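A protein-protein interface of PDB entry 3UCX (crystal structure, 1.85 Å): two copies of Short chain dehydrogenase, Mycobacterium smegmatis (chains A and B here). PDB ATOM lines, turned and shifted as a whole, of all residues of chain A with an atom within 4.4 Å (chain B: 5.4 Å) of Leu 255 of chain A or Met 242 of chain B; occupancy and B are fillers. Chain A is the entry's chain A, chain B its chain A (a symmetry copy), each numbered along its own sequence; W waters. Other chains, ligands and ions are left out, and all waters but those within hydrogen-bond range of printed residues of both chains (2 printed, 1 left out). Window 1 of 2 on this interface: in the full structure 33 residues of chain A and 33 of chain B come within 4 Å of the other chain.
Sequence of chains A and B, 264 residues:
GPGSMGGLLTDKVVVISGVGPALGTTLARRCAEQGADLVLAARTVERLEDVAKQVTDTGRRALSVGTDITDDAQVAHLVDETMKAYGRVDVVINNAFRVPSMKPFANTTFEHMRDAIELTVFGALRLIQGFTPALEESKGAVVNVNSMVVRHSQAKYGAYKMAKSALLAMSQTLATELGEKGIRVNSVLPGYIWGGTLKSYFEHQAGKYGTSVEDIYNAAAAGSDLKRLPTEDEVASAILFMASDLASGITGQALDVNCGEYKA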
ATOM      1  N   SER A 187      -2.335 -29.645  12.116  1.00  0.00           N
ATOM      2  CA  SER A 187      -2.492 -28.658  11.055  1.00  0.00           C
ATOM      3  C   SER A 187      -2.971 -27.325  11.630  1.00  0.00           C
ATOM      4  O   SER A 187      -3.689 -27.283  12.644  1.00  0.00           O
ATOM      5  CB  SER A 187      -3.517 -29.156  10.030  1.00  0.00           C
ATOM      6  OG  SER A 187      -3.158 -30.416   9.464  1.00  0.00           O
ATOM      7  N   VAL A 188      -2.554 -26.233  10.994  1.00  0.00           N
ATOM      8  CA  VAL A 188      -3.058 -24.891  11.302  1.00  0.00           C
ATOM      9  C   VAL A 188      -3.696 -24.344  10.000  1.00  0.00           C
ATOM     10  O   VAL A 188      -3.089 -24.418   8.914  1.00  0.00           O
ATOM     11  CB  VAL A 188      -1.969 -23.962  11.856  1.00  0.00           C
ATOM     12  CG1 VAL A 188      -2.464 -22.507  11.966  1.00  0.00           C
ATOM     13  CG2 VAL A 188      -1.428 -24.468  13.208  1.00  0.00           C
ATOM     14  N   LEU A 189      -4.941 -23.886  10.110  1.00  0.00           N
ATOM     15  CA  LEU A 189      -5.773 -23.510   8.956  1.00  0.00           C
ATOM     16  C   LEU A 189      -6.096 -22.020   9.001  1.00  0.00           C
ATOM     17  O   LEU A 189      -7.092 -21.612   9.580  1.00  0.00           O
ATOM     18  CB  LEU A 189      -7.084 -24.288   8.945  1.00  0.00           C
ATOM     19  CG  LEU A 189      -7.024 -25.747   8.477  1.00  0.00           C
ATOM     20  CD1 LEU A 189      -6.024 -26.539   9.323  1.00  0.00           C
ATOM     21  CD2 LEU A 189      -8.428 -26.356   8.540  1.00  0.00           C
ATOM     22  N   ALA A 238      -0.228 -19.685  16.721  1.00  0.00           N
ATOM     23  CA  ALA A 238      -0.923 -20.985  16.666  1.00  0.00           C
ATOM     24  C   ALA A 238       0.043 -22.112  16.262  1.00  0.00           C
ATOM     25  O   ALA A 238       0.011 -23.198  16.835  1.00  0.00           O
ATOM     26  CB  ALA A 238      -2.078 -20.924  15.679  1.00  0.00           C
ATOM     27  N   MET A 242       1.327 -25.392  18.563  1.00  0.00           N
ATOM     28  CA  MET A 242       1.254 -26.777  18.071  1.00  0.00           C
ATOM     29  C   MET A 242       2.628 -27.448  17.978  1.00  0.00           C
ATOM     30  O   MET A 242       2.735 -28.662  18.160  1.00  0.00           O
ATOM     31  CB  MET A 242       0.588 -26.823  16.699  1.00  0.00           C
ATOM     32  CG  MET A 242      -0.916 -26.639  16.723  1.00  0.00           C
ATOM     33  SD  MET A 242      -1.720 -27.988  17.626  1.00  0.00           S
ATOM     34  CE  MET A 242      -3.388 -27.911  16.963  1.00  0.00           C
ATOM     35  N   GLN A 253      -5.006 -32.947  14.912  1.00  0.00           N
ATOM     36  CA  GLN A 253      -5.989 -31.859  14.984  1.00  0.00           C
ATOM     37  C   GLN A 253      -5.697 -30.761  13.983  1.00  0.00           C
ATOM     38  O   GLN A 253      -4.555 -30.555  13.594  1.00  0.00           O
ATOM     39  CB  GLN A 253      -6.022 -31.245  16.388  1.00  0.00           C
ATOM     40  CG  GLN A 253      -6.277 -32.265  17.484  1.00  0.00           C
ATOM     41  CD  GLN A 253      -7.461 -33.183  17.204  1.00  0.00           C
ATOM     42  OE1 GLN A 253      -8.516 -32.734  16.762  1.00  0.00           O
ATOM     43  NE2 GLN A 253      -7.285 -34.505  17.475  1.00  0.00           N
ATOM     44  N   ALA A 254      -6.764 -30.065  13.579  1.00  0.00           N
ATOM     45  CA  ALA A 254      -6.703 -28.902  12.738  1.00  0.00           C
ATOM     46  C   ALA A 254      -7.127 -27.695  13.603  1.00  0.00           C
ATOM     47  O   ALA A 254      -8.215 -27.678  14.161  1.00  0.00           O
ATOM     48  CB  ALA A 254      -7.665 -29.077  11.550  1.00  0.00           C
ATOM     49  N   LEU A 255      -6.275 -26.696  13.726  1.00  0.00           N
ATOM     50  CA  LEU A 255      -6.620 -25.497  14.505  1.00  0.00           C
ATOM     51  C   LEU A 255      -6.798 -24.345  13.513  1.00  0.00           C
ATOM     52  O   LEU A 255      -5.858 -23.945  12.826  1.00  0.00           O
ATOM     53  CB  LEU A 255      -5.508 -25.193  15.492  1.00  0.00           C
ATOM     54  CG  LEU A 255      -5.607 -23.932  16.370  1.00  0.00           C
ATOM     55  CD1 LEU A 255      -6.886 -23.990  17.196  1.00  0.00           C
ATOM     56  CD2 LEU A 255      -4.381 -23.736  17.264  1.00  0.00           C
ATOM     57  N   ASP A 256      -8.019 -23.853  13.411  1.00  0.00           N
ATOM     58  CA  ASP A 256      -8.362 -22.816  12.445  1.00  0.00           C
ATOM     59  C   ASP A 256      -8.068 -21.465  13.040  1.00  0.00           C
ATOM     60  O   ASP A 256      -8.461 -21.197  14.169  1.00  0.00           O
ATOM     61  CB  ASP A 256      -9.845 -22.897  12.100  1.00  0.00           C
ATOM     62  CG  ASP A 256     -10.211 -24.170  11.335  1.00  0.00           C
ATOM     63  OD1 ASP A 256     -10.114 -25.268  11.918  1.00  0.00           O
ATOM     64  OD2 ASP A 256     -10.617 -24.074  10.165  1.00  0.00           O
ATOM     65  N   VAL A 257      -7.361 -20.627  12.289  1.00  0.00           N
ATOM     66  CA  VAL A 257      -7.005 -19.284  12.746  1.00  0.00           C
ATOM     67  C   VAL A 257      -7.628 -18.342  11.720  1.00  0.00           C
ATOM     68  O   VAL A 257      -7.032 -18.042  10.684  1.00  0.00           O
ATOM     69  CB  VAL A 257      -5.486 -19.081  12.867  1.00  0.00           C
ATOM     70  CG1 VAL A 257      -5.164 -17.700  13.470  1.00  0.00           C
ATOM     71  CG2 VAL A 257      -4.824 -20.178  13.707  1.00  0.00           C
ATOM     72  N   ALA B 141     -11.510 -13.180  26.839  1.00  0.00           N
ATOM     73  CA  ALA B 141     -11.657 -14.485  26.260  1.00  0.00           C
ATOM     74  C   ALA B 141     -12.420 -15.411  27.189  1.00  0.00           C
ATOM     75  O   ALA B 141     -12.268 -15.369  28.417  1.00  0.00           O
ATOM     76  CB  ALA B 141     -10.279 -15.079  25.930  1.00  0.00           C
ATOM     77  N   VAL B 143     -13.096 -19.553  27.639  1.00  0.00           N
ATOM     78  CA  VAL B 143     -12.812 -20.950  27.282  1.00  0.00           C
ATOM     79  C   VAL B 143     -13.794 -21.844  28.004  1.00  0.00           C
ATOM     80  O   VAL B 143     -13.801 -21.909  29.243  1.00  0.00           O
ATOM     81  CB  VAL B 143     -11.382 -21.415  27.634  1.00  0.00           C
ATOM     82  CG1 VAL B 143     -11.126 -22.813  27.043  1.00  0.00           C
ATOM     83  CG2 VAL B 143     -10.343 -20.434  27.120  1.00  0.00           C
ATOM     84  N   ARG B 184     -13.414 -13.159  22.526  1.00  0.00           N
ATOM     85  CA  ARG B 184     -13.172 -14.478  21.926  1.00  0.00           C
ATOM     86  C   ARG B 184     -13.839 -15.563  22.760  1.00  0.00           C
ATOM     87  O   ARG B 184     -13.901 -15.479  23.997  1.00  0.00           O
ATOM     88  CB  ARG B 184     -11.673 -14.753  21.801  1.00  0.00           C
ATOM     89  CG  ARG B 184     -10.967 -13.744  20.912  1.00  0.00           C
ATOM     90  CD  ARG B 184      -9.498 -14.065  20.659  1.00  0.00           C
ATOM     91  NE  ARG B 184      -8.726 -14.174  21.893  1.00  0.00           N
ATOM     92  CZ  ARG B 184      -8.379 -15.319  22.514  1.00  0.00           C
ATOM     93  NH1 ARG B 184      -8.673 -16.530  22.043  1.00  0.00           N
ATOM     94  NH2 ARG B 184      -7.683 -15.238  23.631  1.00  0.00           N
ATOM     95  N   ASN B 186     -13.817 -19.845  22.784  1.00  0.00           N
ATOM     96  CA  ASN B 186     -13.365 -21.139  22.251  1.00  0.00           C
ATOM     97  C   ASN B 186     -13.663 -22.270  23.223  1.00  0.00           C
ATOM     98  O   ASN B 186     -13.967 -22.030  24.412  1.00  0.00           O
ATOM     99  CB  ASN B 186     -11.855 -21.084  21.960  1.00  0.00           C
ATOM    100  CG  ASN B 186     -11.502 -20.088  20.866  1.00  0.00           C
ATOM    101  OD1 ASN B 186     -11.730 -20.351  19.684  1.00  0.00           O
ATOM    102  ND2 ASN B 186     -10.979 -18.916  21.258  1.00  0.00           N
ATOM    103  N   SER B 187     -13.533 -23.501  22.730  1.00  0.00           N
ATOM    104  CA  SER B 187     -13.741 -24.702  23.530  1.00  0.00           C
ATOM    105  C   SER B 187     -12.492 -25.585  23.506  1.00  0.00           C
ATOM    106  O   SER B 187     -11.740 -25.606  22.517  1.00  0.00           O
ATOM    107  CB  SER B 187     -14.926 -25.499  22.973  1.00  0.00           C
ATOM    108  OG  SER B 187     -16.130 -24.734  22.934  1.00  0.00           O
ATOM    109  N   VAL B 188     -12.261 -26.297  24.606  1.00  0.00           N
ATOM    110  CA  VAL B 188     -11.216 -27.322  24.686  1.00  0.00           C
ATOM    111  C   VAL B 188     -11.926 -28.658  25.023  1.00  0.00           C
ATOM    112  O   VAL B 188     -12.763 -28.719  25.944  1.00  0.00           O
ATOM    113  CB  VAL B 188     -10.118 -26.969  25.698  1.00  0.00           C
ATOM    114  CG1 VAL B 188      -9.152 -28.150  25.925  1.00  0.00           C
ATOM    115  CG2 VAL B 188      -9.352 -25.697  25.282  1.00  0.00           C
ATOM    116  N   SER B 237      -2.587 -26.758  29.477  1.00  0.00           N
ATOM    117  CA  SER B 237      -1.811 -25.998  28.491  1.00  0.00           C
ATOM    118  C   SER B 237      -2.664 -25.502  27.305  1.00  0.00           C
ATOM    119  O   SER B 237      -2.493 -24.374  26.833  1.00  0.00           O
ATOM    120  CB  SER B 237      -0.659 -26.836  27.946  1.00  0.00           C
ATOM    121  OG  SER B 237       0.331 -27.066  28.951  1.00  0.00           O
ATOM    122  N   ALA B 238      -3.527 -26.367  26.797  1.00  0.00           N
ATOM    123  CA  ALA B 238      -4.445 -26.012  25.698  1.00  0.00           C
ATOM    124  C   ALA B 238      -5.393 -24.874  26.114  1.00  0.00           C
ATOM    125  O   ALA B 238      -5.639 -23.951  25.343  1.00  0.00           O
ATOM    126  CB  ALA B 238      -5.258 -27.225  25.275  1.00  0.00           C
ATOM    127  N   ILE B 239      -5.913 -24.957  27.333  1.00  0.00           N
ATOM    128  CA  ILE B 239      -6.835 -23.943  27.862  1.00  0.00           C
ATOM    129  C   ILE B 239      -6.105 -22.612  28.041  1.00  0.00           C
ATOM    130  O   ILE B 239      -6.606 -21.553  27.662  1.00  0.00           O
ATOM    131  CB  ILE B 239      -7.463 -24.401  29.191  1.00  0.00           C
ATOM    132  CG1 ILE B 239      -8.384 -25.590  28.951  1.00  0.00           C
ATOM    133  CG2 ILE B 239      -8.213 -23.267  29.881  1.00  0.00           C
ATOM    134  CD1 ILE B 239      -8.745 -26.343  30.214  1.00  0.00           C
ATOM    135  N   LEU B 240      -4.915 -22.664  28.624  1.00  0.00           N
ATOM    136  CA  LEU B 240      -4.079 -21.459  28.759  1.00  0.00           C
ATOM    137  C   LEU B 240      -3.782 -20.794  27.420  1.00  0.00           C
ATOM    138  O   LEU B 240      -3.886 -19.558  27.304  1.00  0.00           O
ATOM    139  CB  LEU B 240      -2.778 -21.764  29.503  1.00  0.00           C
ATOM    140  CG  LEU B 240      -2.851 -21.580  31.025  1.00  0.00           C
ATOM    141  CD1 LEU B 240      -3.903 -22.489  31.662  1.00  0.00           C
ATOM    142  CD2 LEU B 240      -1.466 -21.872  31.582  1.00  0.00           C
ATOM    143  N   PHE B 241      -3.443 -21.589  26.401  1.00  0.00           N
ATOM    144  CA  PHE B 241      -3.205 -21.061  25.057  1.00  0.00           C
ATOM    145  C   PHE B 241      -4.431 -20.295  24.544  1.00  0.00           C
ATOM    146  O   PHE B 241      -4.318 -19.126  24.153  1.00  0.00           O
ATOM    147  CB  PHE B 241      -2.857 -22.181  24.074  1.00  0.00           C
ATOM    148  CG  PHE B 241      -2.940 -21.779  22.637  1.00  0.00           C
ATOM    149  CD1 PHE B 241      -1.982 -20.969  22.076  1.00  0.00           C
ATOM    150  CD2 PHE B 241      -3.988 -22.189  21.860  1.00  0.00           C
ATOM    151  CE1 PHE B 241      -2.059 -20.594  20.729  1.00  0.00           C
ATOM    152  CE2 PHE B 241      -4.088 -21.819  20.529  1.00  0.00           C
ATOM    153  CZ  PHE B 241      -3.110 -21.015  19.972  1.00  0.00           C
ATOM    154  N   MET B 242      -5.589 -20.956  24.593  1.00  0.00           N
ATOM    155  CA  MET B 242      -6.848 -20.352  24.131  1.00  0.00           C
ATOM    156  C   MET B 242      -7.237 -19.103  24.929  1.00  0.00           C
ATOM    157  O   MET B 242      -7.854 -18.189  24.382  1.00  0.00           O
ATOM    158  CB  MET B 242      -7.988 -21.363  24.211  1.00  0.00           C
ATOM    159  CG  MET B 242      -7.970 -22.418  23.122  1.00  0.00           C
ATOM    160  SD  MET B 242      -8.187 -21.667  21.488  1.00  0.00           S
ATOM    161  CE  MET B 242      -8.780 -23.068  20.532  1.00  0.00           C
ATOM    162  N   ALA B 243      -6.884 -19.076  26.217  1.00  0.00           N
ATOM    163  CA  ALA B 243      -7.154 -17.915  27.085  1.00  0.00           C
ATOM    164  C   ALA B 243      -6.210 -16.746  26.829  1.00  0.00           C
ATOM    165  O   ALA B 243      -6.524 -15.602  27.170  1.00  0.00           O
ATOM    166  CB  ALA B 243      -7.084 -18.324  28.558  1.00  0.00           C
ATOM    167  N   SER B 244      -5.064 -17.020  26.226  1.00  0.00           N
ATOM    168  CA  SER B 244      -3.997 -16.065  26.087  1.00  0.00           C
ATOM    169  C   SER B 244      -4.044 -15.290  24.784  1.00  0.00           C
ATOM    170  O   SER B 244      -4.721 -15.663  23.833  1.00  0.00           O
ATOM    171  CB  SER B 244      -2.645 -16.801  26.143  1.00  0.00           C
ATOM    172  OG  SER B 244      -2.338 -17.344  24.867  1.00  0.00           O
ATOM    173  N   ALA B 247      -3.631 -16.690  21.187  1.00  0.00           N
ATOM    174  CA  ALA B 247      -4.800 -17.141  20.458  1.00  0.00           C
ATOM    175  C   ALA B 247      -5.660 -15.940  20.012  1.00  0.00           C
ATOM    176  O   ALA B 247      -6.844 -16.115  19.709  1.00  0.00           O
ATOM    177  CB  ALA B 247      -5.618 -18.086  21.325  1.00  0.00           C
ATOM    178  N   ILE B 250      -7.989 -16.342  17.118  1.00  0.00           N
ATOM    179  CA  ILE B 250      -8.757 -17.591  17.170  1.00  0.00           C
ATOM    180  C   ILE B 250     -10.020 -17.417  17.999  1.00  0.00           C
ATOM    181  O   ILE B 250      -9.975 -17.073  19.188  1.00  0.00           O
ATOM    182  CB  ILE B 250      -7.933 -18.760  17.763  1.00  0.00           C
ATOM    183  CG1 ILE B 250      -6.638 -18.944  16.960  1.00  0.00           C
ATOM    184  CG2 ILE B 250      -8.807 -20.025  17.819  1.00  0.00           C
ATOM    185  CD1 ILE B 250      -5.689 -19.961  17.603  1.00  0.00           C
ATOM    186  N   GLN B 253     -13.668 -21.843  17.925  1.00  0.00           N
ATOM    187  CA  GLN B 253     -13.002 -23.117  17.626  1.00  0.00           C
ATOM    188  C   GLN B 253     -13.059 -24.077  18.796  1.00  0.00           C
ATOM    189  O   GLN B 253     -13.139 -23.661  19.944  1.00  0.00           O
ATOM    190  CB  GLN B 253     -11.533 -22.890  17.250  1.00  0.00           C
ATOM    191  CG  GLN B 253     -11.352 -21.913  16.102  1.00  0.00           C
ATOM    192  CD  GLN B 253     -12.239 -22.208  14.899  1.00  0.00           C
ATOM    193  OE1 GLN B 253     -12.379 -23.357  14.485  1.00  0.00           O
ATOM    194  NE2 GLN B 253     -12.851 -21.142  14.316  1.00  0.00           N
ATOM    195  N   ALA B 254     -13.013 -25.372  18.468  1.00  0.00           N
ATOM    196  CA  ALA B 254     -12.924 -26.446  19.418  1.00  0.00           C
ATOM    197  C   ALA B 254     -11.527 -27.083  19.249  1.00  0.00           C
ATOM    198  O   ALA B 254     -11.171 -27.529  18.167  1.00  0.00           O
ATOM    199  CB  ALA B 254     -14.026 -27.480  19.128  1.00  0.00           C
ATOM    200  N   LEU B 255     -10.736 -27.120  20.303  1.00  0.00           N
ATOM    201  CA  LEU B 255      -9.404 -27.741  20.230  1.00  0.00           C
ATOM    202  C   LEU B 255      -9.456 -29.028  21.056  1.00  0.00           C
ATOM    203  O   LEU B 255      -9.661 -28.997  22.271  1.00  0.00           O
ATOM    204  CB  LEU B 255      -8.365 -26.784  20.783  1.00  0.00           C
ATOM    205  CG  LEU B 255      -6.898 -27.245  20.884  1.00  0.00           C
ATOM    206  CD1 LEU B 255      -6.397 -27.642  19.501  1.00  0.00           C
ATOM    207  CD2 LEU B 255      -5.989 -26.190  21.519  1.00  0.00           C
HETATM  208  O   HOH W   1     -10.206 -19.074  14.352  1.00  0.00           O
HETATM  209  O   HOH W   2      -9.463 -30.160  17.331  1.00  0.00           O
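Water W1 bridges O of Asp 256 of chain A and NE2 of Gln 253 of chain B.
Water W2 lies within hydrogen-bond range of the side-chain amide oxygen of Gln 253 of chain A (2.8 Å) and the backbone carbonyl oxygen of Ala 254 of chain B (3.2 Å).
Ala 238 of chain A touches Phe 241 of chain B (CA to CZ, 3.96 Å).
Met 242 of chain A touches Leu 255 of chain B.
Phe 241 of chain B touches Leu 255 of chain A.
CD1 of Leu 255 of chain A touches CE of Met 242 of chain B, 3.9 Å away.
Asp 256 of chain A touches Ile 250 of chain B (O to CG2, 3.8 Å).
CB of Asp 256 of chain A touches OE1 of Gln 253 of chain B (3.5 Å).
Val 257 of chain A touches Ile 250 of chain B (CG2 to CG1, 3.9 Å).
Of the 10 printed residues of chain A, 5 touch a printed residue of chain B.
Hydrophobic or aromatic side chains of chain B that line the printed part of chain A: Phe 241, Met 242, Ile 250 and Leu 255.
Among the printed residues, 7 pairs touch across the chains.
Met 242 of chain A touches Leu 255 of chain B, and with the chains exchanged Leu 255 of chain A touches Met 242 of chain B.
Of the 7 pairs that touch across the chains among the printed residues, 2 have their exchanged pair printed and touching as well.
The guanidinium group (NH1) of Arg 184 of chain B is in hydrogen-bond range of the backbone carbonyl oxygen (O) of Met 242 of chain B, at 3.0 Å.
The backbone carbonyl oxygen (O) of Ser 187 of chain A is in hydrogen-bond range of the backbone NH (N) of Leu 255 of chain A (2.9 Å).
The backbone carbonyl oxygen (O) of Ser 187 of chain B is in hydrogen-bond range of the backbone NH (N) of Leu 255 of chain B.
O of Phe 241 of chain B lies within hydrogen-bond range of OG of Ser 244 of chain B, 2.8 Å away.
The guanidinium group of Arg 184 of chain B lies within hydrogen-bond range of the backbone carbonyl oxygen of Ile 250 of chain B.
The backbone NH (N) of Ser 187 of chain B lies within hydrogen-bond range of the backbone carbonyl oxygen (O) of Gln 253 of chain B.
Of the printed residues of chain B, Leu 255 of chain A touches Phe 241 and Met 242.
Of chain A, only Leu 255 (3.9 Å) comes within 4 Å of Met 242 of chain B.
Of the printed residues of chain B, Asp 256 of chain A touches Ile 250 and Gln 253.
Of the printed residues of chain A, Ile 250 of chain B touches Asp 256 (3.8 Å) and Val 257 (3.9 Å).
Of the printed residues of chain B, Met 242 of chain A touches Leu 255 (3.9 Å).
Asn 186 of chain B touches none of the printed residues of chain A.
The nearest printed residue of chain B that does not touch Leu 255 of chain A is Ile 250 of chain B (4.01 Å).
The nearest printed residue of chain A that does not touch Ile 250 of chain B is Leu 255 of chain A (4.01 Å).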
